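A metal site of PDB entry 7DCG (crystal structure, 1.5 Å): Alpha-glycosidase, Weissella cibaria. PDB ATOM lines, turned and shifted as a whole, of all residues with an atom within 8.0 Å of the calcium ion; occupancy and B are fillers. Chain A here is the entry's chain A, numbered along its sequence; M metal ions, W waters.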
ATOM      1  N   PRO A 150      15.454 -16.323   4.006  1.00  0.00           N
ATOM      2  CA  PRO A 150      14.759 -15.310   4.853  1.00  0.00           C
ATOM      3  C   PRO A 150      15.523 -14.928   6.132  1.00  0.00           C
ATOM      4  O   PRO A 150      15.377 -13.800   6.625  1.00  0.00           O
ATOM      5  CB  PRO A 150      13.391 -15.988   5.128  1.00  0.00           C
ATOM      6  CG  PRO A 150      13.594 -17.453   4.727  1.00  0.00           C
ATOM      7  CD  PRO A 150      14.621 -17.507   3.694  1.00  0.00           C
ATOM      8  N   GLU A 151      16.354 -15.810   6.695  1.00  0.00           N
ATOM      9  CA  GLU A 151      17.137 -15.435   7.885  1.00  0.00           C
ATOM     10  C   GLU A 151      18.049 -14.245   7.611  1.00  0.00           C
ATOM     11  O   GLU A 151      18.536 -13.592   8.554  1.00  0.00           O
ATOM     12  CB  GLU A 151      17.985 -16.621   8.367  1.00  0.00           C
ATOM     13  CG  GLU A 151      17.923 -16.861   9.896  1.00  0.00           C
ATOM     14  CD  GLU A 151      18.707 -15.883  10.754  1.00  0.00           C
ATOM     15  OE1 GLU A 151      19.935 -15.672  10.475  1.00  0.00           O
ATOM     16  OE2 GLU A 151      18.153 -15.360  11.774  1.00  0.00           O
ATOM     17  N   ALA A 154      16.114  -9.312   5.731  1.00  0.00           N
ATOM     18  CA  ALA A 154      15.904  -8.097   6.521  1.00  0.00           C
ATOM     19  C   ALA A 154      15.292  -8.493   7.868  1.00  0.00           C
ATOM     20  O   ALA A 154      14.335  -9.286   7.904  1.00  0.00           O
ATOM     21  CB  ALA A 154      15.016  -7.058   5.788  1.00  0.00           C
ATOM     22  N   ASN A 155      15.788  -7.892   8.960  1.00  0.00           N
ATOM     23  CA  ASN A 155      15.167  -8.062  10.258  1.00  0.00           C
ATOM     24  C   ASN A 155      14.137  -6.960  10.422  1.00  0.00           C
ATOM     25  O   ASN A 155      14.476  -5.805  10.757  1.00  0.00           O
ATOM     26  CB  ASN A 155      16.245  -8.009  11.351  1.00  0.00           C
ATOM     27  CG  ASN A 155      15.703  -8.356  12.737  1.00  0.00           C
ATOM     28  OD1 ASN A 155      14.517  -8.668  12.894  1.00  0.00           O
ATOM     29  ND2 ASN A 155      16.580  -8.328  13.740  1.00  0.00           N
ATOM     30  N   GLY A 156      12.859  -7.295  10.201  1.00  0.00           N
ATOM     31  CA  GLY A 156      11.773  -6.357  10.417  1.00  0.00           C
ATOM     32  C   GLY A 156      11.190  -6.384  11.808  1.00  0.00           C
ATOM     33  O   GLY A 156      10.272  -5.609  12.120  1.00  0.00           O
ATOM     34  N   ASP A 157      11.721  -7.226  12.706  1.00  0.00           N
ATOM     35  CA  ASP A 157      11.117  -7.333  14.044  1.00  0.00           C
ATOM     36  C   ASP A 157      12.167  -7.945  14.957  1.00  0.00           C
ATOM     37  O   ASP A 157      12.364  -9.168  14.936  1.00  0.00           O
ATOM     38  CB  ASP A 157       9.858  -8.205  13.950  1.00  0.00           C
ATOM     39  CG  ASP A 157       9.124  -8.324  15.252  1.00  0.00           C
ATOM     40  OD1 ASP A 157       9.637  -7.805  16.292  1.00  0.00           O
ATOM     41  OD2 ASP A 157       8.031  -8.948  15.288  1.00  0.00           O
ATOM     42  N   VAL A 158      12.814  -7.122  15.817  1.00  0.00           N
ATOM     43  CA  VAL A 158      13.809  -7.708  16.739  1.00  0.00           C
ATOM     44  C   VAL A 158      13.163  -8.608  17.799  1.00  0.00           C
ATOM     45  O   VAL A 158      13.874  -9.427  18.424  1.00  0.00           O
ATOM     46  CB  VAL A 158      14.635  -6.635  17.475  1.00  0.00           C
ATOM     47  CG1 VAL A 158      15.535  -5.885  16.488  1.00  0.00           C
ATOM     48  CG2 VAL A 158      13.695  -5.680  18.284  1.00  0.00           C
ATOM     49  N   SER A 159      11.864  -8.463  18.046  1.00  0.00           N
ATOM     50  CA  SER A 159      11.238  -9.185  19.152  1.00  0.00           C
ATOM     51  C   SER A 159      11.082 -10.677  18.896  1.00  0.00           C
ATOM     52  O   SER A 159      10.887 -11.426  19.861  1.00  0.00           O
ATOM     53  CB  SER A 159       9.894  -8.528  19.476  1.00  0.00           C
ATOM     54  OG  SER A 159       8.874  -8.923  18.590  1.00  0.00           O
ATOM     55  N   ASN A 160      11.242 -11.132  17.647  1.00  0.00           N
ATOM     56  CA  ASN A 160      11.179 -12.548  17.353  1.00  0.00           C
ATOM     57  C   ASN A 160      12.554 -13.131  17.096  1.00  0.00           C
ATOM     58  O   ASN A 160      12.639 -14.278  16.642  1.00  0.00           O
ATOM     59  CB  ASN A 160      10.246 -12.858  16.188  1.00  0.00           C
ATOM     60  CG  ASN A 160      10.679 -12.199  14.905  1.00  0.00           C
ATOM     61  OD1 ASN A 160      11.874 -11.875  14.745  1.00  0.00           O
ATOM     62  ND2 ASN A 160       9.732 -12.061  13.926  1.00  0.00           N
ATOM     63  N   ASP A 161      13.633 -12.403  17.427  1.00  0.00           N
ATOM     64  CA  ASP A 161      14.981 -12.870  17.074  1.00  0.00           C
ATOM     65  C   ASP A 161      15.381 -14.093  17.915  1.00  0.00           C
ATOM     66  O   ASP A 161      15.086 -14.141  19.124  1.00  0.00           O
ATOM     67  CB  ASP A 161      16.041 -11.755  17.299  1.00  0.00           C
ATOM     68  CG  ASP A 161      15.964 -10.636  16.255  1.00  0.00           C
ATOM     69  OD1 ASP A 161      15.188 -10.783  15.271  1.00  0.00           O
ATOM     70  OD2 ASP A 161      16.681  -9.610  16.458  1.00  0.00           O
ATOM     71  N   PRO A 162      16.086 -15.029  17.310  1.00  0.00           N
ATOM     72  CA  PRO A 162      16.656 -16.146  18.051  1.00  0.00           C
ATOM     73  C   PRO A 162      17.580 -15.675  19.161  1.00  0.00           C
ATOM     74  O   PRO A 162      18.189 -14.612  19.073  1.00  0.00           O
ATOM     75  CB  PRO A 162      17.445 -16.912  16.966  1.00  0.00           C
ATOM     76  CG  PRO A 162      16.733 -16.563  15.691  1.00  0.00           C
ATOM     77  CD  PRO A 162      16.284 -15.147  15.838  1.00  0.00           C
ATOM     78  N   THR A 165      21.308 -13.794  18.528  1.00  0.00           N
ATOM     79  CA  THR A 165      21.335 -13.052  17.267  1.00  0.00           C
ATOM     80  C   THR A 165      22.441 -12.011  17.263  1.00  0.00           C
ATOM     81  O   THR A 165      22.597 -11.228  18.217  1.00  0.00           O
ATOM     82  CB  THR A 165      19.952 -12.382  17.038  1.00  0.00           C
ATOM     83  OG1 THR A 165      18.971 -13.408  16.793  1.00  0.00           O
ATOM     84  CG2 THR A 165      19.963 -11.436  15.801  1.00  0.00           C
ATOM     85  N   TRP A 168      23.449  -6.884  12.642  1.00  0.00           N
ATOM     86  CA  TRP A 168      23.310  -7.009  11.182  1.00  0.00           C
ATOM     87  C   TRP A 168      24.535  -6.415  10.515  1.00  0.00           C
ATOM     88  O   TRP A 168      24.802  -5.212  10.647  1.00  0.00           O
ATOM     89  CB  TRP A 168      22.053  -6.244  10.710  1.00  0.00           C
ATOM     90  CG  TRP A 168      21.629  -6.684   9.348  1.00  0.00           C
ATOM     91  CD1 TRP A 168      22.093  -6.210   8.139  1.00  0.00           C
ATOM     92  CD2 TRP A 168      20.685  -7.700   9.046  1.00  0.00           C
ATOM     93  NE1 TRP A 168      21.491  -6.887   7.078  1.00  0.00           N
ATOM     94  CE2 TRP A 168      20.615  -7.811   7.625  1.00  0.00           C
ATOM     95  CE3 TRP A 168      19.914  -8.574   9.840  1.00  0.00           C
ATOM     96  CZ2 TRP A 168      19.795  -8.733   6.987  1.00  0.00           C
ATOM     97  CZ3 TRP A 168      19.091  -9.531   9.189  1.00  0.00           C
ATOM     98  CH2 TRP A 168      19.021  -9.578   7.775  1.00  0.00           C
ATOM     99  N   TYR A 180      20.985 -13.926  12.413  1.00  0.00           N
ATOM    100  CA  TYR A 180      20.977 -12.477  12.259  1.00  0.00           C
ATOM    101  C   TYR A 180      19.571 -11.877  12.399  1.00  0.00           C
ATOM    102  O   TYR A 180      19.428 -10.633  12.418  1.00  0.00           O
ATOM    103  CB  TYR A 180      21.600 -12.081  10.903  1.00  0.00           C
ATOM    104  CG  TYR A 180      23.061 -12.266  10.902  1.00  0.00           C
ATOM    105  CD1 TYR A 180      23.906 -11.255  11.342  1.00  0.00           C
ATOM    106  CD2 TYR A 180      23.630 -13.477  10.484  1.00  0.00           C
ATOM    107  CE1 TYR A 180      25.280 -11.418  11.334  1.00  0.00           C
ATOM    108  CE2 TYR A 180      25.001 -13.652  10.441  1.00  0.00           C
ATOM    109  CZ  TYR A 180      25.829 -12.616  10.891  1.00  0.00           C
ATOM    110  OH  TYR A 180      27.188 -12.773  10.843  1.00  0.00           O
ATOM    111  N   GLY A 181      18.535 -12.700  12.484  1.00  0.00           N
ATOM    112  CA  GLY A 181      17.210 -12.188  12.841  1.00  0.00           C
ATOM    113  C   GLY A 181      16.307 -11.858  11.668  1.00  0.00           C
ATOM    114  O   GLY A 181      15.248 -11.239  11.874  1.00  0.00           O
ATOM    115  N   GLY A 182      16.679 -12.230  10.449  1.00  0.00           N
ATOM    116  CA  GLY A 182      15.833 -11.913   9.303  1.00  0.00           C
ATOM    117  C   GLY A 182      14.491 -12.624   9.408  1.00  0.00           C
ATOM    118  O   GLY A 182      14.416 -13.695   9.983  1.00  0.00           O
ATOM    119  N   ASP A 183      13.416 -12.006   8.879  1.00  0.00           N
ATOM    120  CA  ASP A 183      12.093 -12.571   9.110  1.00  0.00           C
ATOM    121  C   ASP A 183      11.121 -12.057   8.041  1.00  0.00           C
ATOM    122  O   ASP A 183      11.498 -11.340   7.089  1.00  0.00           O
ATOM    123  CB  ASP A 183      11.596 -12.169  10.522  1.00  0.00           C
ATOM    124  CG  ASP A 183      11.741 -10.641  10.773  1.00  0.00           C
ATOM    125  OD1 ASP A 183      11.529  -9.849   9.866  1.00  0.00           O
ATOM    126  OD2 ASP A 183      12.030 -10.261  11.907  1.00  0.00           O
ATOM    127  N   LEU A 184       9.855 -12.494   8.155  1.00  0.00           N
ATOM    128  CA  LEU A 184       8.888 -12.124   7.114  1.00  0.00           C
ATOM    129  C   LEU A 184       8.561 -10.646   7.149  1.00  0.00           C
ATOM    130  O   LEU A 184       8.260 -10.065   6.092  1.00  0.00           O
ATOM    131  CB  LEU A 184       7.573 -12.910   7.281  1.00  0.00           C
ATOM    132  CG  LEU A 184       7.667 -14.419   7.141  1.00  0.00           C
ATOM    133  CD1 LEU A 184       6.214 -14.997   7.193  1.00  0.00           C
ATOM    134  CD2 LEU A 184       8.322 -14.805   5.833  1.00  0.00           C
ATOM    135  N   GLN A 185       8.539 -10.019   8.332  1.00  0.00           N
ATOM    136  CA  GLN A 185       8.245  -8.589   8.332  1.00  0.00           C
ATOM    137  C   GLN A 185       9.327  -7.833   7.581  1.00  0.00           C
ATOM    138  O   GLN A 185       9.030  -6.838   6.903  1.00  0.00           O
ATOM    139  CB  GLN A 185       8.135  -8.077   9.774  1.00  0.00           C
ATOM    140  CG  GLN A 185       7.777  -6.568   9.870  1.00  0.00           C
ATOM    141  CD  GLN A 185       6.416  -6.285   9.281  1.00  0.00           C
ATOM    142  OE1 GLN A 185       5.414  -6.915   9.675  1.00  0.00           O
ATOM    143  NE2 GLN A 185       6.352  -5.320   8.364  1.00  0.00           N
ATOM    144  N   GLY A 186      10.566  -8.325   7.632  1.00  0.00           N
ATOM    145  CA  GLY A 186      11.626  -7.690   6.849  1.00  0.00           C
ATOM    146  C   GLY A 186      11.387  -7.770   5.355  1.00  0.00           C
ATOM    147  O   GLY A 186      11.669  -6.809   4.604  1.00  0.00           O
ATOM    148  N   PRO A 226       8.261 -19.457  14.189  1.00  0.00           N
ATOM    149  CA  PRO A 226       7.877 -18.263  14.957  1.00  0.00           C
ATOM    150  C   PRO A 226       8.984 -17.216  15.010  1.00  0.00           C
ATOM    151  O   PRO A 226       8.693 -16.065  15.369  1.00  0.00           O
ATOM    152  CB  PRO A 226       7.511 -18.808  16.336  1.00  0.00           C
ATOM    153  CG  PRO A 226       8.100 -20.136  16.388  1.00  0.00           C
ATOM    154  CD  PRO A 226       8.236 -20.689  14.992  1.00  0.00           C
ATOM    155  N   HIS A 227      10.211 -17.555  14.633  1.00  0.00           N
ATOM    156  CA  HIS A 227      11.212 -16.494  14.510  1.00  0.00           C
ATOM    157  C   HIS A 227      11.042 -15.732  13.209  1.00  0.00           C
ATOM    158  O   HIS A 227      11.637 -14.675  13.059  1.00  0.00           O
ATOM    159  CB  HIS A 227      12.628 -17.086  14.561  1.00  0.00           C
ATOM    160  CG  HIS A 227      12.880 -17.819  15.826  1.00  0.00           C
ATOM    161  ND1 HIS A 227      12.709 -19.179  15.944  1.00  0.00           N
ATOM    162  CD2 HIS A 227      13.181 -17.363  17.058  1.00  0.00           C
ATOM    163  CE1 HIS A 227      12.912 -19.533  17.202  1.00  0.00           C
ATOM    164  NE2 HIS A 227      13.223 -18.454  17.900  1.00  0.00           N
ATOM    165  N   PHE A 228      10.311 -16.285  12.263  1.00  0.00           N
ATOM    166  CA  PHE A 228      10.003 -15.579  11.021  1.00  0.00           C
ATOM    167  C   PHE A 228       8.677 -14.840  11.047  1.00  0.00           C
ATOM    168  O   PHE A 228       8.523 -13.823  10.353  1.00  0.00           O
ATOM    169  CB  PHE A 228       9.975 -16.579   9.847  1.00  0.00           C
ATOM    170  CG  PHE A 228      11.333 -17.076   9.384  1.00  0.00           C
ATOM    171  CD1 PHE A 228      12.512 -16.491   9.835  1.00  0.00           C
ATOM    172  CD2 PHE A 228      11.412 -18.141   8.479  1.00  0.00           C
ATOM    173  CE1 PHE A 228      13.783 -16.949   9.365  1.00  0.00           C
ATOM    174  CE2 PHE A 228      12.663 -18.587   7.984  1.00  0.00           C
ATOM    175  CZ  PHE A 228      13.855 -18.003   8.440  1.00  0.00           C
ATOM    176  N   GLY A 229       7.693 -15.352  11.768  1.00  0.00           N
ATOM    177  CA  GLY A 229       6.380 -14.713  11.728  1.00  0.00           C
ATOM    178  C   GLY A 229       5.309 -15.721  12.120  1.00  0.00           C
ATOM    179  O   GLY A 229       5.573 -16.657  12.854  1.00  0.00           O
HETATM  180 CA    CA M   1      13.626 -10.780  13.605  1.00  0.00          CA
HETATM  181  O   HOH W   1      13.905 -13.245  13.489  1.00  0.00           O
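The backbone carbonyl oxygen of His 227 sits close to the side-chain amide nitrogen of Asn 160, 3.3 Å away. OD1 of Asp 183 lies within hydrogen-bond range of N of Gly 156 (2.9 Å). The backbone carbonyl oxygen (O) of Ala 154 sits at hydrogen-bond distance from the backbone NH (N) of Asp 183 (3.0 Å). N of Gly 186 lies within hydrogen-bond range of OD1 of Asp 183, at 2.9 Å. The backbone NH (N) of Gln 185 sits close to the side-chain carboxylate (OD1) of Asp 183 (3.4 Å). The backbone NH (N) of Asp 183 lies within hydrogen-bond range of the backbone carbonyl oxygen (O) of Pro 150. The backbone NH (N) of Gly 181 sits at hydrogen-bond distance from the side-chain carboxylate (OE2) of Glu 151 (2.8 Å). OD1 of Asp 157 sits at hydrogen-bond distance from OG of Ser 159, 2.7 Å away.
The calcium ion is bound by the side-chain carboxylate (OD1) of Asp 161, 2.3 Å away. The side-chain amide oxygen (OD1) of Asn 160 is bound to the calcium ion, 2.4 Å away. OD2 of Asp 183 binds the calcium ion (2.4 Å). The calcium ion is bound by OD1 of Asn 155. O of Gly 181 is bound to the calcium ion (2.4 Å). The backbone carbonyl oxygen (O) of Asp 157 is bound to the calcium ion, 2.4 Å away. Water W1 is bound to the calcium ion.
Within 4 Å of the calcium ion: Asn 155, Asp 157, Asn 160, Asp 161, Gly 181 and Asp 183.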
